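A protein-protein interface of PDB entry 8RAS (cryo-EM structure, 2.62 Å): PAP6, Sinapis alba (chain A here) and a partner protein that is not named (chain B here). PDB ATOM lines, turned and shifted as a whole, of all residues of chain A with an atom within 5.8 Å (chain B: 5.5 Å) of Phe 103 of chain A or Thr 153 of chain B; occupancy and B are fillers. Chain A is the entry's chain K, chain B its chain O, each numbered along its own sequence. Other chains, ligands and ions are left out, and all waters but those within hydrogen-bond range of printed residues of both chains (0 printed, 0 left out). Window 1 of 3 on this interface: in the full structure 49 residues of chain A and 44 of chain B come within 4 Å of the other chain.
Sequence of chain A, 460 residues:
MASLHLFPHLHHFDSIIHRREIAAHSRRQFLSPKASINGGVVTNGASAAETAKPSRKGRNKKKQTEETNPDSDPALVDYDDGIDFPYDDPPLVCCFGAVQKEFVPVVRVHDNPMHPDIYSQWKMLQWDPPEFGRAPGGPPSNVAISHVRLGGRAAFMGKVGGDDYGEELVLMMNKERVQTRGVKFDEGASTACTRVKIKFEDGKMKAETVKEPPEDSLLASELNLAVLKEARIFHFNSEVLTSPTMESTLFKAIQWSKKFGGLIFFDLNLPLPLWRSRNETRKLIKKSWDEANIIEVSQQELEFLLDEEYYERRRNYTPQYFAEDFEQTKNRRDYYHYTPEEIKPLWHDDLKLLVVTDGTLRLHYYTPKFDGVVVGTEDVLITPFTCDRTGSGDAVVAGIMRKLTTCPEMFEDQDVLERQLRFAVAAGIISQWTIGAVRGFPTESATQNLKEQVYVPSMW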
ATOM      1  N   GLN A 100     -17.021 -16.651  21.702  1.00  0.00           N
ATOM      2  CA  GLN A 100     -17.498 -17.109  22.995  1.00  0.00           C
ATOM      3  C   GLN A 100     -16.874 -16.255  24.087  1.00  0.00           C
ATOM      4  O   GLN A 100     -15.817 -15.647  23.900  1.00  0.00           O
ATOM      5  CB  GLN A 100     -17.167 -18.589  23.228  1.00  0.00           C
ATOM      6  CG  GLN A 100     -17.907 -19.544  22.310  1.00  0.00           C
ATOM      7  CD  GLN A 100     -17.134 -20.819  22.050  1.00  0.00           C
ATOM      8  OE1 GLN A 100     -16.092 -20.805  21.396  1.00  0.00           O
ATOM      9  NE2 GLN A 100     -17.641 -21.931  22.564  1.00  0.00           N
ATOM     10  N   LYS A 101     -17.544 -16.213  25.233  1.00  0.00           N
ATOM     11  CA  LYS A 101     -17.022 -15.527  26.405  1.00  0.00           C
ATOM     12  C   LYS A 101     -16.218 -16.520  27.234  1.00  0.00           C
ATOM     13  O   LYS A 101     -16.773 -17.503  27.739  1.00  0.00           O
ATOM     14  CB  LYS A 101     -18.156 -14.915  27.227  1.00  0.00           C
ATOM     15  CG  LYS A 101     -18.366 -13.434  26.961  1.00  0.00           C
ATOM     16  CD  LYS A 101     -19.396 -12.832  27.900  1.00  0.00           C
ATOM     17  CE  LYS A 101     -19.024 -13.059  29.355  1.00  0.00           C
ATOM     18  NZ  LYS A 101     -20.213 -12.956  30.245  1.00  0.00           N
ATOM     19  N   GLU A 102     -14.912 -16.267  27.351  1.00  0.00           N
ATOM     20  CA  GLU A 102     -13.970 -17.140  28.046  1.00  0.00           C
ATOM     21  C   GLU A 102     -13.848 -18.477  27.323  1.00  0.00           C
ATOM     22  O   GLU A 102     -13.398 -18.518  26.173  1.00  0.00           O
ATOM     23  CB  GLU A 102     -14.384 -17.335  29.506  1.00  0.00           C
ATOM     24  CG  GLU A 102     -13.771 -16.315  30.450  1.00  0.00           C
ATOM     25  CD  GLU A 102     -14.019 -14.888  30.004  1.00  0.00           C
ATOM     26  OE1 GLU A 102     -15.193 -14.535  29.768  1.00  0.00           O
ATOM     27  OE2 GLU A 102     -13.041 -14.121  29.884  1.00  0.00           O
ATOM     28  N   PHE A 103     -14.235 -19.570  27.982  1.00  0.00           N
ATOM     29  CA  PHE A 103     -14.299 -20.899  27.368  1.00  0.00           C
ATOM     30  C   PHE A 103     -12.937 -21.339  26.819  1.00  0.00           C
ATOM     31  O   PHE A 103     -12.699 -21.385  25.611  1.00  0.00           O
ATOM     32  CB  PHE A 103     -15.370 -20.963  26.273  1.00  0.00           C
ATOM     33  CG  PHE A 103     -15.626 -22.356  25.777  1.00  0.00           C
ATOM     34  CD1 PHE A 103     -16.385 -23.239  26.521  1.00  0.00           C
ATOM     35  CD2 PHE A 103     -15.094 -22.788  24.575  1.00  0.00           C
ATOM     36  CE1 PHE A 103     -16.612 -24.520  26.075  1.00  0.00           C
ATOM     37  CE2 PHE A 103     -15.318 -24.068  24.126  1.00  0.00           C
ATOM     38  CZ  PHE A 103     -16.080 -24.934  24.874  1.00  0.00           C
ATOM     39  N   VAL A 104     -12.028 -21.621  27.746  1.00  0.00           N
ATOM     40  CA  VAL A 104     -10.775 -22.263  27.328  1.00  0.00           C
ATOM     41  C   VAL A 104     -11.082 -23.639  26.741  1.00  0.00           C
ATOM     42  O   VAL A 104     -11.810 -24.436  27.363  1.00  0.00           O
ATOM     43  CB  VAL A 104      -9.789 -22.357  28.510  1.00  0.00           C
ATOM     44  CG1 VAL A 104     -10.349 -23.206  29.640  1.00  0.00           C
ATOM     45  CG2 VAL A 104      -8.456 -22.913  28.040  1.00  0.00           C
ATOM     46  N   PRO A 105     -10.604 -23.956  25.533  1.00  0.00           N
ATOM     47  CA  PRO A 105     -10.906 -25.265  24.935  1.00  0.00           C
ATOM     48  C   PRO A 105     -10.032 -26.404  25.442  1.00  0.00           C
ATOM     49  O   PRO A 105     -10.505 -27.537  25.568  1.00  0.00           O
ATOM     50  CB  PRO A 105     -10.673 -25.022  23.441  1.00  0.00           C
ATOM     51  CG  PRO A 105      -9.678 -23.923  23.397  1.00  0.00           C
ATOM     52  CD  PRO A 105      -9.991 -23.033  24.563  1.00  0.00           C
ATOM     53  N   GLY A 137      -5.125 -20.715  25.435  1.00  0.00           N
ATOM     54  CA  GLY A 137      -5.787 -19.985  24.379  1.00  0.00           C
ATOM     55  C   GLY A 137      -7.300 -20.024  24.539  1.00  0.00           C
ATOM     56  O   GLY A 137      -7.847 -20.559  25.501  1.00  0.00           O
ATOM     57  N   GLY A 138      -7.982 -19.439  23.560  1.00  0.00           N
ATOM     58  CA  GLY A 138      -9.423 -19.396  23.580  1.00  0.00           C
ATOM     59  C   GLY A 138     -10.029 -19.294  22.197  1.00  0.00           C
ATOM     60  O   GLY A 138      -9.438 -19.717  21.198  1.00  0.00           O
ATOM     61  N   PRO A 139     -11.230 -18.733  22.120  1.00  0.00           N
ATOM     62  CA  PRO A 139     -11.895 -18.561  20.827  1.00  0.00           C
ATOM     63  C   PRO A 139     -11.161 -17.547  19.968  1.00  0.00           C
ATOM     64  O   PRO A 139     -10.394 -16.723  20.487  1.00  0.00           O
ATOM     65  CB  PRO A 139     -13.294 -18.057  21.213  1.00  0.00           C
ATOM     66  CG  PRO A 139     -13.134 -17.491  22.581  1.00  0.00           C
ATOM     67  CD  PRO A 139     -12.082 -18.316  23.244  1.00  0.00           C
ATOM     68  N   GLU A 239     -11.083 -26.039  16.832  1.00  0.00           N
ATOM     69  CA  GLU A 239     -12.436 -26.256  17.328  1.00  0.00           C
ATOM     70  C   GLU A 239     -13.430 -26.427  16.187  1.00  0.00           C
ATOM     71  O   GLU A 239     -14.402 -27.179  16.320  1.00  0.00           O
ATOM     72  CB  GLU A 239     -12.853 -25.094  18.227  1.00  0.00           C
ATOM     73  CG  GLU A 239     -14.068 -25.376  19.090  1.00  0.00           C
ATOM     74  CD  GLU A 239     -15.361 -24.924  18.439  1.00  0.00           C
ATOM     75  OE1 GLU A 239     -15.330 -23.942  17.668  1.00  0.00           O
ATOM     76  OE2 GLU A 239     -16.408 -25.549  18.698  1.00  0.00           O
ATOM     77  N   VAL B 101     -26.479 -29.199  35.038  1.00  0.00           N
ATOM     78  CA  VAL B 101     -25.216 -29.879  35.296  1.00  0.00           C
ATOM     79  C   VAL B 101     -24.077 -28.973  34.859  1.00  0.00           C
ATOM     80  O   VAL B 101     -24.045 -28.512  33.713  1.00  0.00           O
ATOM     81  CB  VAL B 101     -25.146 -31.234  34.572  1.00  0.00           C
ATOM     82  CG1 VAL B 101     -23.875 -31.966  34.954  1.00  0.00           C
ATOM     83  CG2 VAL B 101     -26.368 -32.070  34.901  1.00  0.00           C
ATOM     84  N   ASP B 102     -23.142 -28.722  35.770  1.00  0.00           N
ATOM     85  CA  ASP B 102     -21.976 -27.894  35.507  1.00  0.00           C
ATOM     86  C   ASP B 102     -20.736 -28.766  35.405  1.00  0.00           C
ATOM     87  O   ASP B 102     -20.507 -29.629  36.259  1.00  0.00           O
ATOM     88  CB  ASP B 102     -21.784 -26.851  36.607  1.00  0.00           C
ATOM     89  CG  ASP B 102     -20.602 -25.940  36.343  1.00  0.00           C
ATOM     90  OD1 ASP B 102     -20.397 -25.550  35.175  1.00  0.00           O
ATOM     91  OD2 ASP B 102     -19.877 -25.614  37.305  1.00  0.00           O
ATOM     92  N   PHE B 103     -19.943 -28.545  34.366  1.00  0.00           N
ATOM     93  CA  PHE B 103     -18.652 -29.197  34.209  1.00  0.00           C
ATOM     94  C   PHE B 103     -17.572 -28.160  34.478  1.00  0.00           C
ATOM     95  O   PHE B 103     -17.554 -27.101  33.843  1.00  0.00           O
ATOM     96  CB  PHE B 103     -18.510 -29.802  32.814  1.00  0.00           C
ATOM     97  CG  PHE B 103     -19.307 -31.060  32.622  1.00  0.00           C
ATOM     98  CD1 PHE B 103     -20.664 -31.000  32.354  1.00  0.00           C
ATOM     99  CD2 PHE B 103     -18.703 -32.300  32.719  1.00  0.00           C
ATOM    100  CE1 PHE B 103     -21.401 -32.153  32.181  1.00  0.00           C
ATOM    101  CE2 PHE B 103     -19.436 -33.457  32.546  1.00  0.00           C
ATOM    102  CZ  PHE B 103     -20.786 -33.383  32.277  1.00  0.00           C
ATOM    103  N   PRO B 110     -11.863 -19.244  34.408  1.00  0.00           N
ATOM    104  CA  PRO B 110     -13.276 -18.871  34.235  1.00  0.00           C
ATOM    105  C   PRO B 110     -14.239 -19.640  35.124  1.00  0.00           C
ATOM    106  O   PRO B 110     -15.366 -19.177  35.326  1.00  0.00           O
ATOM    107  CB  PRO B 110     -13.535 -19.165  32.753  1.00  0.00           C
ATOM    108  CG  PRO B 110     -12.218 -19.007  32.115  1.00  0.00           C
ATOM    109  CD  PRO B 110     -11.200 -19.464  33.109  1.00  0.00           C
ATOM    110  N   GLN B 147     -19.995 -34.972  25.177  1.00  0.00           N
ATOM    111  CA  GLN B 147     -19.710 -33.921  24.200  1.00  0.00           C
ATOM    112  C   GLN B 147     -19.399 -32.591  24.891  1.00  0.00           C
ATOM    113  O   GLN B 147     -20.035 -31.565  24.647  1.00  0.00           O
ATOM    114  CB  GLN B 147     -20.860 -33.767  23.198  1.00  0.00           C
ATOM    115  CG  GLN B 147     -21.381 -35.072  22.628  1.00  0.00           C
ATOM    116  CD  GLN B 147     -20.327 -35.830  21.851  1.00  0.00           C
ATOM    117  OE1 GLN B 147     -20.062 -37.000  22.123  1.00  0.00           O
ATOM    118  NE2 GLN B 147     -19.719 -35.165  20.878  1.00  0.00           N
ATOM    119  N   VAL B 148     -18.401 -32.631  25.765  1.00  0.00           N
ATOM    120  CA  VAL B 148     -17.866 -31.435  26.406  1.00  0.00           C
ATOM    121  C   VAL B 148     -16.572 -31.071  25.692  1.00  0.00           C
ATOM    122  O   VAL B 148     -15.621 -31.859  25.675  1.00  0.00           O
ATOM    123  CB  VAL B 148     -17.632 -31.653  27.908  1.00  0.00           C
ATOM    124  CG1 VAL B 148     -16.913 -30.462  28.510  1.00  0.00           C
ATOM    125  CG2 VAL B 148     -18.950 -31.898  28.619  1.00  0.00           C
ATOM    126  N   ARG B 149     -16.539 -29.883  25.092  1.00  0.00           N
ATOM    127  CA  ARG B 149     -15.392 -29.432  24.318  1.00  0.00           C
ATOM    128  C   ARG B 149     -14.521 -28.429  25.060  1.00  0.00           C
ATOM    129  O   ARG B 149     -13.472 -28.039  24.539  1.00  0.00           O
ATOM    130  CB  ARG B 149     -15.861 -28.815  22.997  1.00  0.00           C
ATOM    131  CG  ARG B 149     -16.529 -29.800  22.060  1.00  0.00           C
ATOM    132  CD  ARG B 149     -16.852 -29.154  20.728  1.00  0.00           C
ATOM    133  NE  ARG B 149     -18.015 -28.281  20.818  1.00  0.00           N
ATOM    134  CZ  ARG B 149     -18.437 -27.497  19.837  1.00  0.00           C
ATOM    135  NH1 ARG B 149     -17.814 -27.452  18.672  1.00  0.00           N
ATOM    136  NH2 ARG B 149     -19.512 -26.738  20.030  1.00  0.00           N
ATOM    137  N   GLY B 150     -14.925 -28.006  26.248  1.00  0.00           N
ATOM    138  CA  GLY B 150     -14.157 -27.036  27.003  1.00  0.00           C
ATOM    139  C   GLY B 150     -14.907 -26.656  28.257  1.00  0.00           C
ATOM    140  O   GLY B 150     -15.983 -27.187  28.551  1.00  0.00           O
ATOM    141  N   LEU B 151     -14.324 -25.721  28.996  1.00  0.00           N
ATOM    142  CA  LEU B 151     -14.906 -25.247  30.238  1.00  0.00           C
ATOM    143  C   LEU B 151     -14.967 -23.728  30.233  1.00  0.00           C
ATOM    144  O   LEU B 151     -14.087 -23.073  29.669  1.00  0.00           O
ATOM    145  CB  LEU B 151     -14.089 -25.724  31.447  1.00  0.00           C
ATOM    146  CG  LEU B 151     -13.818 -27.225  31.540  1.00  0.00           C
ATOM    147  CD1 LEU B 151     -12.686 -27.500  32.509  1.00  0.00           C
ATOM    148  CD2 LEU B 151     -15.070 -27.971  31.951  1.00  0.00           C
ATOM    149  N   PRO B 152     -15.993 -23.138  30.859  1.00  0.00           N
ATOM    150  CA  PRO B 152     -17.135 -23.782  31.531  1.00  0.00           C
ATOM    151  C   PRO B 152     -18.191 -24.302  30.556  1.00  0.00           C
ATOM    152  O   PRO B 152     -18.433 -23.704  29.514  1.00  0.00           O
ATOM    153  CB  PRO B 152     -17.687 -22.658  32.417  1.00  0.00           C
ATOM    154  CG  PRO B 152     -17.327 -21.399  31.693  1.00  0.00           C
ATOM    155  CD  PRO B 152     -15.996 -21.677  31.052  1.00  0.00           C
ATOM    156  N   THR B 153     -18.832 -25.422  30.880  1.00  0.00           N
ATOM    157  CA  THR B 153     -19.876 -26.009  30.050  1.00  0.00           C
ATOM    158  C   THR B 153     -21.052 -26.387  30.936  1.00  0.00           C
ATOM    159  O   THR B 153     -20.869 -27.036  31.969  1.00  0.00           O
ATOM    160  CB  THR B 153     -19.362 -27.239  29.293  1.00  0.00           C
ATOM    161  OG1 THR B 153     -18.504 -26.822  28.224  1.00  0.00           O
ATOM    162  CG2 THR B 153     -20.520 -28.040  28.718  1.00  0.00           C
ATOM    163  N   LEU B 154     -22.253 -25.984  30.530  1.00  0.00           N
ATOM    164  CA  LEU B 154     -23.470 -26.249  31.282  1.00  0.00           C
ATOM    165  C   LEU B 154     -24.402 -27.132  30.466  1.00  0.00           C
ATOM    166  O   LEU B 154     -24.493 -26.991  29.243  1.00  0.00           O
ATOM    167  CB  LEU B 154     -24.188 -24.948  31.651  1.00  0.00           C
ATOM    168  CG  LEU B 154     -23.610 -24.125  32.801  1.00  0.00           C
ATOM    169  CD1 LEU B 154     -24.373 -22.821  32.953  1.00  0.00           C
ATOM    170  CD2 LEU B 154     -23.649 -24.918  34.089  1.00  0.00           C
ATOM    171  N   PHE B 155     -25.091 -28.041  31.149  1.00  0.00           N
ATOM    172  CA  PHE B 155     -26.098 -28.900  30.538  1.00  0.00           C
ATOM    173  C   PHE B 155     -27.427 -28.667  31.237  1.00  0.00           C
ATOM    174  O   PHE B 155     -27.542 -28.883  32.447  1.00  0.00           O
ATOM    175  CB  PHE B 155     -25.698 -30.373  30.626  1.00  0.00           C
ATOM    176  CG  PHE B 155     -24.750 -30.806  29.550  1.00  0.00           C
ATOM    177  CD1 PHE B 155     -25.227 -31.288  28.344  1.00  0.00           C
ATOM    178  CD2 PHE B 155     -23.383 -30.726  29.739  1.00  0.00           C
ATOM    179  CE1 PHE B 155     -24.357 -31.685  27.350  1.00  0.00           C
ATOM    180  CE2 PHE B 155     -22.509 -31.122  28.749  1.00  0.00           C
ATOM    181  CZ  PHE B 155     -22.997 -31.600  27.554  1.00  0.00           C
ATOM    182  N   ARG B 167     -26.890 -27.711  25.755  1.00  0.00           N
ATOM    183  CA  ARG B 167     -25.525 -27.483  26.207  1.00  0.00           C
ATOM    184  C   ARG B 167     -25.126 -26.056  25.854  1.00  0.00           C
ATOM    185  O   ARG B 167     -25.215 -25.653  24.690  1.00  0.00           O
ATOM    186  CB  ARG B 167     -24.561 -28.483  25.569  1.00  0.00           C
ATOM    187  CG  ARG B 167     -23.119 -28.311  26.011  1.00  0.00           C
ATOM    188  CD  ARG B 167     -22.162 -29.013  25.069  1.00  0.00           C
ATOM    189  NE  ARG B 167     -22.118 -28.369  23.763  1.00  0.00           N
ATOM    190  CZ  ARG B 167     -21.604 -28.922  22.673  1.00  0.00           C
ATOM    191  NH1 ARG B 167     -21.071 -30.131  22.698  1.00  0.00           N
ATOM    192  NH2 ARG B 167     -21.630 -28.246  21.528  1.00  0.00           N
ATOM    193  N   THR B 168     -24.690 -25.300  26.857  1.00  0.00           N
ATOM    194  CA  THR B 168     -24.213 -23.938  26.668  1.00  0.00           C
ATOM    195  C   THR B 168     -22.732 -23.866  27.009  1.00  0.00           C
ATOM    196  O   THR B 168     -22.293 -24.402  28.031  1.00  0.00           O
ATOM    197  CB  THR B 168     -24.995 -22.946  27.534  1.00  0.00           C
ATOM    198  OG1 THR B 168     -24.858 -23.301  28.915  1.00  0.00           O
ATOM    199  CG2 THR B 168     -26.465 -22.960  27.160  1.00  0.00           C
ATOM    200  N   GLU B 169     -21.964 -23.203  26.150  1.00  0.00           N
ATOM    201  CA  GLU B 169     -20.520 -23.105  26.298  1.00  0.00           C
ATOM    202  C   GLU B 169     -20.126 -21.650  26.497  1.00  0.00           C
ATOM    203  O   GLU B 169     -20.556 -20.777  25.738  1.00  0.00           O
ATOM    204  CB  GLU B 169     -19.810 -23.692  25.077  1.00  0.00           C
ATOM    205  CG  GLU B 169     -20.218 -25.122  24.770  1.00  0.00           C
ATOM    206  CD  GLU B 169     -19.234 -25.832  23.864  1.00  0.00           C
ATOM    207  OE1 GLU B 169     -19.112 -25.429  22.690  1.00  0.00           O
ATOM    208  OE2 GLU B 169     -18.590 -26.798  24.324  1.00  0.00           O
ATOM    209  N   GLY B 170     -19.314 -21.396  27.512  1.00  0.00           N
ATOM    210  CA  GLY B 170     -18.842 -20.065  27.828  1.00  0.00           C
ATOM    211  C   GLY B 170     -19.498 -19.507  29.080  1.00  0.00           C
ATOM    212  O   GLY B 170     -20.398 -20.100  29.675  1.00  0.00           O
ATOM    213  N   LEU B 171     -19.014 -18.329  29.475  1.00  0.00           N
ATOM    214  CA  LEU B 171     -19.526 -17.625  30.649  1.00  0.00           C
ATOM    215  C   LEU B 171     -20.790 -16.868  30.251  1.00  0.00           C
ATOM    216  O   LEU B 171     -20.792 -15.655  30.038  1.00  0.00           O
ATOM    217  CB  LEU B 171     -18.470 -16.688  31.218  1.00  0.00           C
ATOM    218  CG  LEU B 171     -17.798 -17.077  32.535  1.00  0.00           C
ATOM    219  CD1 LEU B 171     -16.925 -15.938  33.028  1.00  0.00           C
ATOM    220  CD2 LEU B 171     -18.831 -17.450  33.579  1.00  0.00           C
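O of Leu 171 of chain B sits at hydrogen-bond distance from NZ of Lys 101 of chain A (2.8 Å). The backbone NH (N) of Val 104 of chain A is in hydrogen-bond range of the backbone carbonyl oxygen (O) of Leu 151 of chain B (3.2 Å). The guanidinium group of Arg 149 of chain B lies within salt-bridge range of the side-chain carboxylate of Glu 239 of chain A, at 3.6 Å. The backbone carbonyl oxygen of Arg 149 of chain B lies close to the backbone carbonyl oxygen of Pro 105 of chain A (3.2 Å).
N of Phe 103 of chain B sits at hydrogen-bond distance from O of Thr 153 of chain B. OE1 of Glu 169 of chain B lies within salt-bridge range of NH2 of Arg 149 of chain B, 3.0 Å away. The side-chain hydroxyl (OG1) of Thr 153 of chain B sits at hydrogen-bond distance from the backbone carbonyl oxygen (O) of Gly 150 of chain B (2.6 Å). The backbone carbonyl oxygen of Pro 152 of chain B is in hydrogen-bond range of the backbone NH of Gly 170 of chain B. NE of Arg 167 of chain B lies within salt-bridge range of OE2 of Glu 169 of chain B, 3.9 Å away.
Among the printed residues, pairs that only touch across the chains: Phe 103 of chain A with Leu 151 of chain B (3.2 Å), Phe 103 of chain A with Glu 169 of chain B (3.2 Å), Lys 101 of chain A with Gly 170 of chain B (3.3 Å), Phe 103 of chain A with Gly 150 of chain B (3.5 Å), Val 104 of chain A with Gly 150 of chain B (3.5 Å), Glu 102 of chain A with Pro 110 of chain B (3.5 Å), Phe 103 of chain A with Gly 170 of chain B (3.6 Å), Phe 103 of chain A with Pro 152 of chain B (3.7 Å), Phe 103 of chain A with Thr 153 of chain B (3.7 Å), Gln 100 of chain A with Glu 169 of chain B (3.8 Å), Phe 103 of chain A with Arg 149 of chain B (3.8 Å), Glu 102 of chain A with Leu 171 of chain B (3.9 Å) and Pro 105 of chain A with Gly 150 of chain B (3.96 Å).
Of chain A, only Phe 103 comes within 4 Å of Thr 153 of chain B. Of the printed residues of chain B, Gln 100 of chain A touches Glu 169 (3.8 Å). Printed residues of chain B within 4 Å of Lys 101 of chain A: Gly 170 (3.3 Å) and Leu 171 (2.8 Å). Of the printed residues of chain A, Leu 171 of chain B touches Lys 101 (2.8 Å) and Glu 102 (3.9 Å). Printed residues of chain A within 4 Å of Leu 151 of chain B: Phe 103 (3.2 Å) and Val 104 (3.2 Å). Of the printed residues of chain A, Pro 152 of chain B touches Phe 103. Gln 147 of chain B touches none of the printed residues of chain A. Phe 155 of chain B touches none of the printed residues of chain A. The nearest residue of chain B that does not touch Phe 103 of chain A is Pro 110 of chain B (4.6 Å).
Printed residues of chain B that touch a printed residue of chain A: Pro 110, Arg 149, Gly 150, Leu 151, Pro 152, Thr 153, Glu 169, Gly 170 and Leu 171. Hydrophobic or aromatic side chains of chain B that line the printed part of chain A: Pro 110 and Leu 171. Among the printed residues, Asp or Glu carboxylates within 4 Å of a Lys or Arg side-chain nitrogen of the other chain: Glu 239 of chain A with Arg 149 of chain B (2.4 Å).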
